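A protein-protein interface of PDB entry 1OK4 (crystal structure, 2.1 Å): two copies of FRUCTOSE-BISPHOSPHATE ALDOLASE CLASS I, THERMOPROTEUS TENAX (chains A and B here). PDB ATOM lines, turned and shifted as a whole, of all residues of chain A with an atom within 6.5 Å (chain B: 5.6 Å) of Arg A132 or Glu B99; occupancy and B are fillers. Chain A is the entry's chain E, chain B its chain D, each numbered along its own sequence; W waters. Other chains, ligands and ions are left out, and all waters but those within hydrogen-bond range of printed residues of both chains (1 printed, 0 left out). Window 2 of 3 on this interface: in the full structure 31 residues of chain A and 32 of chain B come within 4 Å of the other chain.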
ATOM      1  N   LEU A 127     -23.411  24.987  22.636  1.00  0.00           N
ATOM      2  CA  LEU A 127     -24.198  23.789  22.797  1.00  0.00           C
ATOM      3  C   LEU A 127     -23.411  22.524  22.469  1.00  0.00           C
ATOM      4  O   LEU A 127     -23.608  21.486  23.122  1.00  0.00           O
ATOM      5  CB  LEU A 127     -25.476  23.852  21.946  1.00  0.00           C
ATOM      6  CG  LEU A 127     -26.456  22.704  22.160  1.00  0.00           C
ATOM      7  CD1 LEU A 127     -26.860  22.574  23.644  1.00  0.00           C
ATOM      8  CD2 LEU A 127     -27.707  22.884  21.310  1.00  0.00           C
ATOM      9  N   ALA A 128     -22.550  22.592  21.458  1.00  0.00           N
ATOM     10  CA  ALA A 128     -21.675  21.476  21.100  1.00  0.00           C
ATOM     11  C   ALA A 128     -20.828  21.015  22.297  1.00  0.00           C
ATOM     12  O   ALA A 128     -20.663  19.820  22.518  1.00  0.00           O
ATOM     13  CB  ALA A 128     -20.750  21.879  19.959  1.00  0.00           C
ATOM     14  N   ARG A 129     -20.255  21.969  23.029  1.00  0.00           N
ATOM     15  CA  ARG A 129     -19.432  21.650  24.192  1.00  0.00           C
ATOM     16  C   ARG A 129     -20.286  21.104  25.315  1.00  0.00           C
ATOM     17  O   ARG A 129     -19.900  20.125  25.933  1.00  0.00           O
ATOM     18  CB  ARG A 129     -18.633  22.866  24.677  1.00  0.00           C
ATOM     19  CG  ARG A 129     -17.523  23.286  23.675  1.00  0.00           C
ATOM     20  CD  ARG A 129     -16.579  24.404  24.179  1.00  0.00           C
ATOM     21  NE  ARG A 129     -16.815  25.660  23.466  1.00  0.00           N
ATOM     22  CZ  ARG A 129     -17.517  26.708  23.927  1.00  0.00           C
ATOM     23  NH1 ARG A 129     -18.093  26.697  25.140  1.00  0.00           N
ATOM     24  NH2 ARG A 129     -17.644  27.793  23.156  1.00  0.00           N
ATOM     25  N   ILE A 130     -21.418  21.734  25.576  1.00  0.00           N
ATOM     26  CA  ILE A 130     -22.341  21.263  26.605  1.00  0.00           C
ATOM     27  C   ILE A 130     -22.862  19.860  26.297  1.00  0.00           C
ATOM     28  O   ILE A 130     -22.935  19.017  27.185  1.00  0.00           O
ATOM     29  CB  ILE A 130     -23.469  22.275  26.784  1.00  0.00           C
ATOM     30  CG1 ILE A 130     -22.925  23.499  27.525  1.00  0.00           C
ATOM     31  CG2 ILE A 130     -24.671  21.668  27.535  1.00  0.00           C
ATOM     32  CD1 ILE A 130     -23.695  24.715  27.257  1.00  0.00           C
ATOM     33  N   LYS A 131     -23.217  19.596  25.044  1.00  0.00           N
ATOM     34  CA  LYS A 131     -23.691  18.255  24.656  1.00  0.00           C
ATOM     35  C   LYS A 131     -22.602  17.214  24.923  1.00  0.00           C
ATOM     36  O   LYS A 131     -22.873  16.145  25.451  1.00  0.00           O
ATOM     37  CB  LYS A 131     -24.097  18.228  23.188  1.00  0.00           C
ATOM     38  CG  LYS A 131     -24.396  16.850  22.598  1.00  0.00           C
ATOM     39  CD  LYS A 131     -25.549  16.140  23.299  1.00  0.00           C
ATOM     40  CE  LYS A 131     -25.800  14.774  22.670  1.00  0.00           C
ATOM     41  NZ  LYS A 131     -27.005  14.061  23.290  1.00  0.00           N
ATOM     42  N   ARG A 132     -21.359  17.543  24.584  1.00  0.00           N
ATOM     43  CA  ARG A 132     -20.249  16.610  24.772  1.00  0.00           C
ATOM     44  C   ARG A 132     -20.034  16.307  26.256  1.00  0.00           C
ATOM     45  O   ARG A 132     -19.752  15.150  26.638  1.00  0.00           O
ATOM     46  CB  ARG A 132     -18.979  17.199  24.182  1.00  0.00           C
ATOM     47  CG  ARG A 132     -17.733  16.312  24.279  1.00  0.00           C
ATOM     48  CD  ARG A 132     -16.531  16.988  23.648  1.00  0.00           C
ATOM     49  NE  ARG A 132     -15.550  16.005  23.181  1.00  0.00           N
ATOM     50  CZ  ARG A 132     -14.614  16.224  22.262  1.00  0.00           C
ATOM     51  NH1 ARG A 132     -14.485  17.414  21.674  1.00  0.00           N
ATOM     52  NH2 ARG A 132     -13.783  15.242  21.937  1.00  0.00           N
ATOM     53  N   ASP A 133     -20.163  17.341  27.090  1.00  0.00           N
ATOM     54  CA  ASP A 133     -20.070  17.184  28.546  1.00  0.00           C
ATOM     55  C   ASP A 133     -21.278  16.452  29.147  1.00  0.00           C
ATOM     56  O   ASP A 133     -21.127  15.683  30.091  1.00  0.00           O
ATOM     57  CB  ASP A 133     -19.967  18.541  29.219  1.00  0.00           C
ATOM     58  CG  ASP A 133     -18.553  19.127  29.183  1.00  0.00           C
ATOM     59  OD1 ASP A 133     -17.593  18.417  28.801  1.00  0.00           O
ATOM     60  OD2 ASP A 133     -18.321  20.294  29.559  1.00  0.00           O
ATOM     61  N   ALA A 134     -22.467  16.702  28.626  1.00  0.00           N
ATOM     62  CA  ALA A 134     -23.675  15.959  29.076  1.00  0.00           C
ATOM     63  C   ALA A 134     -23.511  14.459  28.861  1.00  0.00           C
ATOM     64  O   ALA A 134     -23.879  13.643  29.739  1.00  0.00           O
ATOM     65  CB  ALA A 134     -24.889  16.451  28.367  1.00  0.00           C
ATOM     66  N   VAL A 135     -22.982  14.067  27.701  1.00  0.00           N
ATOM     67  CA  VAL A 135     -22.710  12.663  27.432  1.00  0.00           C
ATOM     68  C   VAL A 135     -21.659  12.127  28.397  1.00  0.00           C
ATOM     69  O   VAL A 135     -21.795  11.051  28.934  1.00  0.00           O
ATOM     70  CB  VAL A 135     -22.231  12.449  25.981  1.00  0.00           C
ATOM     71  CG1 VAL A 135     -21.718  11.011  25.749  1.00  0.00           C
ATOM     72  CG2 VAL A 135     -23.371  12.752  25.003  1.00  0.00           C
ATOM     73  N   LYS A 136     -20.609  12.900  28.623  1.00  0.00           N
ATOM     74  CA  LYS A 136     -19.514  12.488  29.497  1.00  0.00           C
ATOM     75  C   LYS A 136     -19.951  12.277  30.955  1.00  0.00           C
ATOM     76  O   LYS A 136     -19.515  11.327  31.600  1.00  0.00           O
ATOM     77  CB  LYS A 136     -18.398  13.522  29.397  1.00  0.00           C
ATOM     78  CG  LYS A 136     -17.301  13.465  30.430  1.00  0.00           C
ATOM     79  CD  LYS A 136     -16.186  14.509  30.092  1.00  0.00           C
ATOM     80  CE  LYS A 136     -15.319  14.824  31.311  1.00  0.00           C
ATOM     81  NZ  LYS A 136     -14.154  15.767  31.023  1.00  0.00           N
ATOM     82  N   PHE A 137     -20.792  13.174  31.454  1.00  0.00           N
ATOM     83  CA  PHE A 137     -21.290  13.107  32.817  1.00  0.00           C
ATOM     84  C   PHE A 137     -22.599  12.336  32.922  1.00  0.00           C
ATOM     85  O   PHE A 137     -23.144  12.245  34.002  1.00  0.00           O
ATOM     86  CB  PHE A 137     -21.450  14.492  33.418  1.00  0.00           C
ATOM     87  CG  PHE A 137     -20.149  15.132  33.766  1.00  0.00           C
ATOM     88  CD1 PHE A 137     -19.537  14.860  34.978  1.00  0.00           C
ATOM     89  CD2 PHE A 137     -19.496  15.970  32.852  1.00  0.00           C
ATOM     90  CE1 PHE A 137     -18.319  15.438  35.307  1.00  0.00           C
ATOM     91  CE2 PHE A 137     -18.289  16.546  33.166  1.00  0.00           C
ATOM     92  CZ  PHE A 137     -17.683  16.264  34.399  1.00  0.00           C
ATOM     93  N   ARG B  62     -25.402  15.153  14.022  1.00  0.00           N
ATOM     94  CA  ARG B  62     -25.058  14.318  15.161  1.00  0.00           C
ATOM     95  C   ARG B  62     -26.266  13.753  15.883  1.00  0.00           C
ATOM     96  O   ARG B  62     -26.216  12.608  16.335  1.00  0.00           O
ATOM     97  CB  ARG B  62     -24.197  15.063  16.171  1.00  0.00           C
ATOM     98  CG  ARG B  62     -24.909  16.263  16.844  1.00  0.00           C
ATOM     99  CD  ARG B  62     -24.180  16.866  18.033  1.00  0.00           C
ATOM    100  NE  ARG B  62     -23.715  15.828  18.941  1.00  0.00           N
ATOM    101  CZ  ARG B  62     -22.641  15.919  19.711  1.00  0.00           C
ATOM    102  NH1 ARG B  62     -21.889  17.029  19.762  1.00  0.00           N
ATOM    103  NH2 ARG B  62     -22.319  14.888  20.454  1.00  0.00           N
ATOM    104  N   SER B  97     -17.692  17.344  17.188  1.00  0.00           N
ATOM    105  CA  SER B  97     -16.279  17.122  16.896  1.00  0.00           C
ATOM    106  C   SER B  97     -16.091  15.838  16.099  1.00  0.00           C
ATOM    107  O   SER B  97     -16.973  14.983  16.049  1.00  0.00           O
ATOM    108  CB  SER B  97     -15.489  17.014  18.192  1.00  0.00           C
ATOM    109  OG  SER B  97     -15.820  15.814  18.908  1.00  0.00           O
ATOM    110  N   VAL B  98     -14.920  15.701  15.494  1.00  0.00           N
ATOM    111  CA  VAL B  98     -14.563  14.502  14.761  1.00  0.00           C
ATOM    112  C   VAL B  98     -14.512  13.305  15.700  1.00  0.00           C
ATOM    113  O   VAL B  98     -14.988  12.211  15.345  1.00  0.00           O
ATOM    114  CB  VAL B  98     -13.198  14.673  14.043  1.00  0.00           C
ATOM    115  CG1 VAL B  98     -12.695  13.351  13.504  1.00  0.00           C
ATOM    116  CG2 VAL B  98     -13.316  15.682  12.926  1.00  0.00           C
ATOM    117  N   GLU B  99     -13.956  13.503  16.892  1.00  0.00           N
ATOM    118  CA  GLU B  99     -13.858  12.432  17.866  1.00  0.00           C
ATOM    119  C   GLU B  99     -15.239  11.851  18.202  1.00  0.00           C
ATOM    120  O   GLU B  99     -15.391  10.634  18.271  1.00  0.00           O
ATOM    121  CB  GLU B  99     -13.147  12.898  19.152  1.00  0.00           C
ATOM    122  CG  GLU B  99     -13.085  11.813  20.228  1.00  0.00           C
ATOM    123  CD  GLU B  99     -12.273  12.214  21.445  1.00  0.00           C
ATOM    124  OE1 GLU B  99     -11.503  13.206  21.378  1.00  0.00           O
ATOM    125  OE2 GLU B  99     -12.367  11.526  22.466  1.00  0.00           O
ATOM    126  N   GLU B 100     -16.227  12.721  18.393  1.00  0.00           N
ATOM    127  CA  GLU B 100     -17.597  12.289  18.646  1.00  0.00           C
ATOM    128  C   GLU B 100     -18.199  11.602  17.430  1.00  0.00           C
ATOM    129  O   GLU B 100     -18.958  10.619  17.560  1.00  0.00           O
ATOM    130  CB  GLU B 100     -18.490  13.456  19.072  1.00  0.00           C
ATOM    131  CG  GLU B 100     -18.186  14.004  20.458  1.00  0.00           C
ATOM    132  CD  GLU B 100     -18.798  15.385  20.673  1.00  0.00           C
ATOM    133  OE1 GLU B 100     -18.312  16.381  20.030  1.00  0.00           O
ATOM    134  OE2 GLU B 100     -19.751  15.463  21.488  1.00  0.00           O
ATOM    135  N   ALA B 101     -17.881  12.092  16.248  1.00  0.00           N
ATOM    136  CA  ALA B 101     -18.345  11.446  15.017  1.00  0.00           C
ATOM    137  C   ALA B 101     -17.878   9.990  14.955  1.00  0.00           C
ATOM    138  O   ALA B 101     -18.656   9.086  14.627  1.00  0.00           O
ATOM    139  CB  ALA B 101     -17.896  12.206  13.794  1.00  0.00           C
ATOM    140  N   VAL B 102     -16.619   9.772  15.299  1.00  0.00           N
ATOM    141  CA  VAL B 102     -16.039   8.441  15.330  1.00  0.00           C
ATOM    142  C   VAL B 102     -16.832   7.540  16.289  1.00  0.00           C
ATOM    143  O   VAL B 102     -17.121   6.396  15.963  1.00  0.00           O
ATOM    144  CB  VAL B 102     -14.558   8.490  15.754  1.00  0.00           C
ATOM    145  CG1 VAL B 102     -14.023   7.109  16.031  1.00  0.00           C
ATOM    146  CG2 VAL B 102     -13.707   9.163  14.683  1.00  0.00           C
ATOM    147  N   SER B 103     -17.191   8.066  17.461  1.00  0.00           N
ATOM    148  CA  SER B 103     -17.915   7.281  18.440  1.00  0.00           C
ATOM    149  C   SER B 103     -19.372   7.012  18.010  1.00  0.00           C
ATOM    150  O   SER B 103     -19.972   6.052  18.448  1.00  0.00           O
ATOM    151  CB  SER B 103     -17.846   7.946  19.824  1.00  0.00           C
ATOM    152  OG  SER B 103     -18.931   8.835  20.015  1.00  0.00           O
ATOM    153  N   LEU B 104     -19.923   7.848  17.133  1.00  0.00           N
ATOM    154  CA  LEU B 104     -21.258   7.631  16.600  1.00  0.00           C
ATOM    155  C   LEU B 104     -21.289   6.699  15.390  1.00  0.00           C
ATOM    156  O   LEU B 104     -22.365   6.430  14.847  1.00  0.00           O
ATOM    157  CB  LEU B 104     -21.910   8.966  16.241  1.00  0.00           C
ATOM    158  CG  LEU B 104     -22.148   9.901  17.420  1.00  0.00           C
ATOM    159  CD1 LEU B 104     -22.458  11.306  16.945  1.00  0.00           C
ATOM    160  CD2 LEU B 104     -23.281   9.371  18.298  1.00  0.00           C
ATOM    161  N   ASP B 133      -8.074  16.923  12.898  1.00  0.00           N
ATOM    162  CA  ASP B 133      -8.700  15.811  13.595  1.00  0.00           C
ATOM    163  C   ASP B 133      -9.073  14.669  12.652  1.00  0.00           C
ATOM    164  O   ASP B 133      -8.934  13.518  13.013  1.00  0.00           O
ATOM    165  CB  ASP B 133      -9.966  16.267  14.319  1.00  0.00           C
ATOM    166  CG  ASP B 133      -9.678  16.966  15.641  1.00  0.00           C
ATOM    167  OD1 ASP B 133      -8.524  16.922  16.125  1.00  0.00           O
ATOM    168  OD2 ASP B 133     -10.576  17.566  16.288  1.00  0.00           O
ATOM    169  N   PHE B 137      -7.857  10.905  13.275  1.00  0.00           N
ATOM    170  CA  PHE B 137      -8.803   9.789  13.468  1.00  0.00           C
ATOM    171  C   PHE B 137      -8.990   8.958  12.192  1.00  0.00           C
ATOM    172  O   PHE B 137      -9.762   8.002  12.189  1.00  0.00           O
ATOM    173  CB  PHE B 137     -10.163  10.293  13.960  1.00  0.00           C
ATOM    174  CG  PHE B 137     -10.159  10.725  15.399  1.00  0.00           C
ATOM    175  CD1 PHE B 137     -10.354   9.800  16.409  1.00  0.00           C
ATOM    176  CD2 PHE B 137      -9.931  12.049  15.747  1.00  0.00           C
ATOM    177  CE1 PHE B 137     -10.313  10.190  17.729  1.00  0.00           C
ATOM    178  CE2 PHE B 137      -9.903  12.446  17.066  1.00  0.00           C
ATOM    179  CZ  PHE B 137     -10.086  11.511  18.056  1.00  0.00           C
HETATM  180  O   HOH W   1     -18.834  18.814  20.508  1.00  0.00           O
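2 positions are printed for both chains. Of the 4 pairs that touch across the chains among the printed residues, none has its exchanged pair printed and touching as well.
Water W1 bridges OE1 of Glu B100 and O of Ala A128.
Among the printed residues, Asp or Glu carboxylates within 4 Å of a Lys or Arg side-chain nitrogen of the other chain: Arg A132 with Glu B99 (3.1 Å).
The guanidinium group of Arg A132 sits at hydrogen-bond distance from the side-chain hydroxyl of Ser B97 (3.5 Å). The side-chain carboxylate of Glu B99 is in salt-bridge range of the guanidinium group of Arg A132 (3.1 Å).
The side-chain hydroxyl (OG) of Ser B103 lies within hydrogen-bond range of the backbone carbonyl oxygen (O) of Glu B100. NH2 of Arg B62 is in salt-bridge range of OE2 of Glu B100 (2.8 Å). OG of Ser B97 is in hydrogen-bond range of OE1 of Glu B100.
Arg B62 touches Lys A131 (CZ to CG, 3.5 Å). Glu B100 touches Arg A132.
Leu A127 touches none of the printed residues of chain B. Of the printed residues of chain B, Lys A131 touches Arg B62 (3.5 Å). Arg A132 touches just these residues of chain B: Ser B97 (3.5 Å), Glu B99 (3.1 Å) and Glu B100 (3.3 Å). Printed residues of chain A within 4 Å of Arg B62: Lys A131 (3.5 Å). Printed residues of chain A within 4 Å of Ser B97: Arg A132 (3.5 Å). Glu B99 touches just one residue of chain A: Arg A132 (3.1 Å). Printed residues of chain A within 4 Å of Glu B100: Arg A132. Phe B137 touches none of the printed residues of chain A. The nearest printed residue of chain A that does not touch Arg B62 is Ala A128 (4.1 Å).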
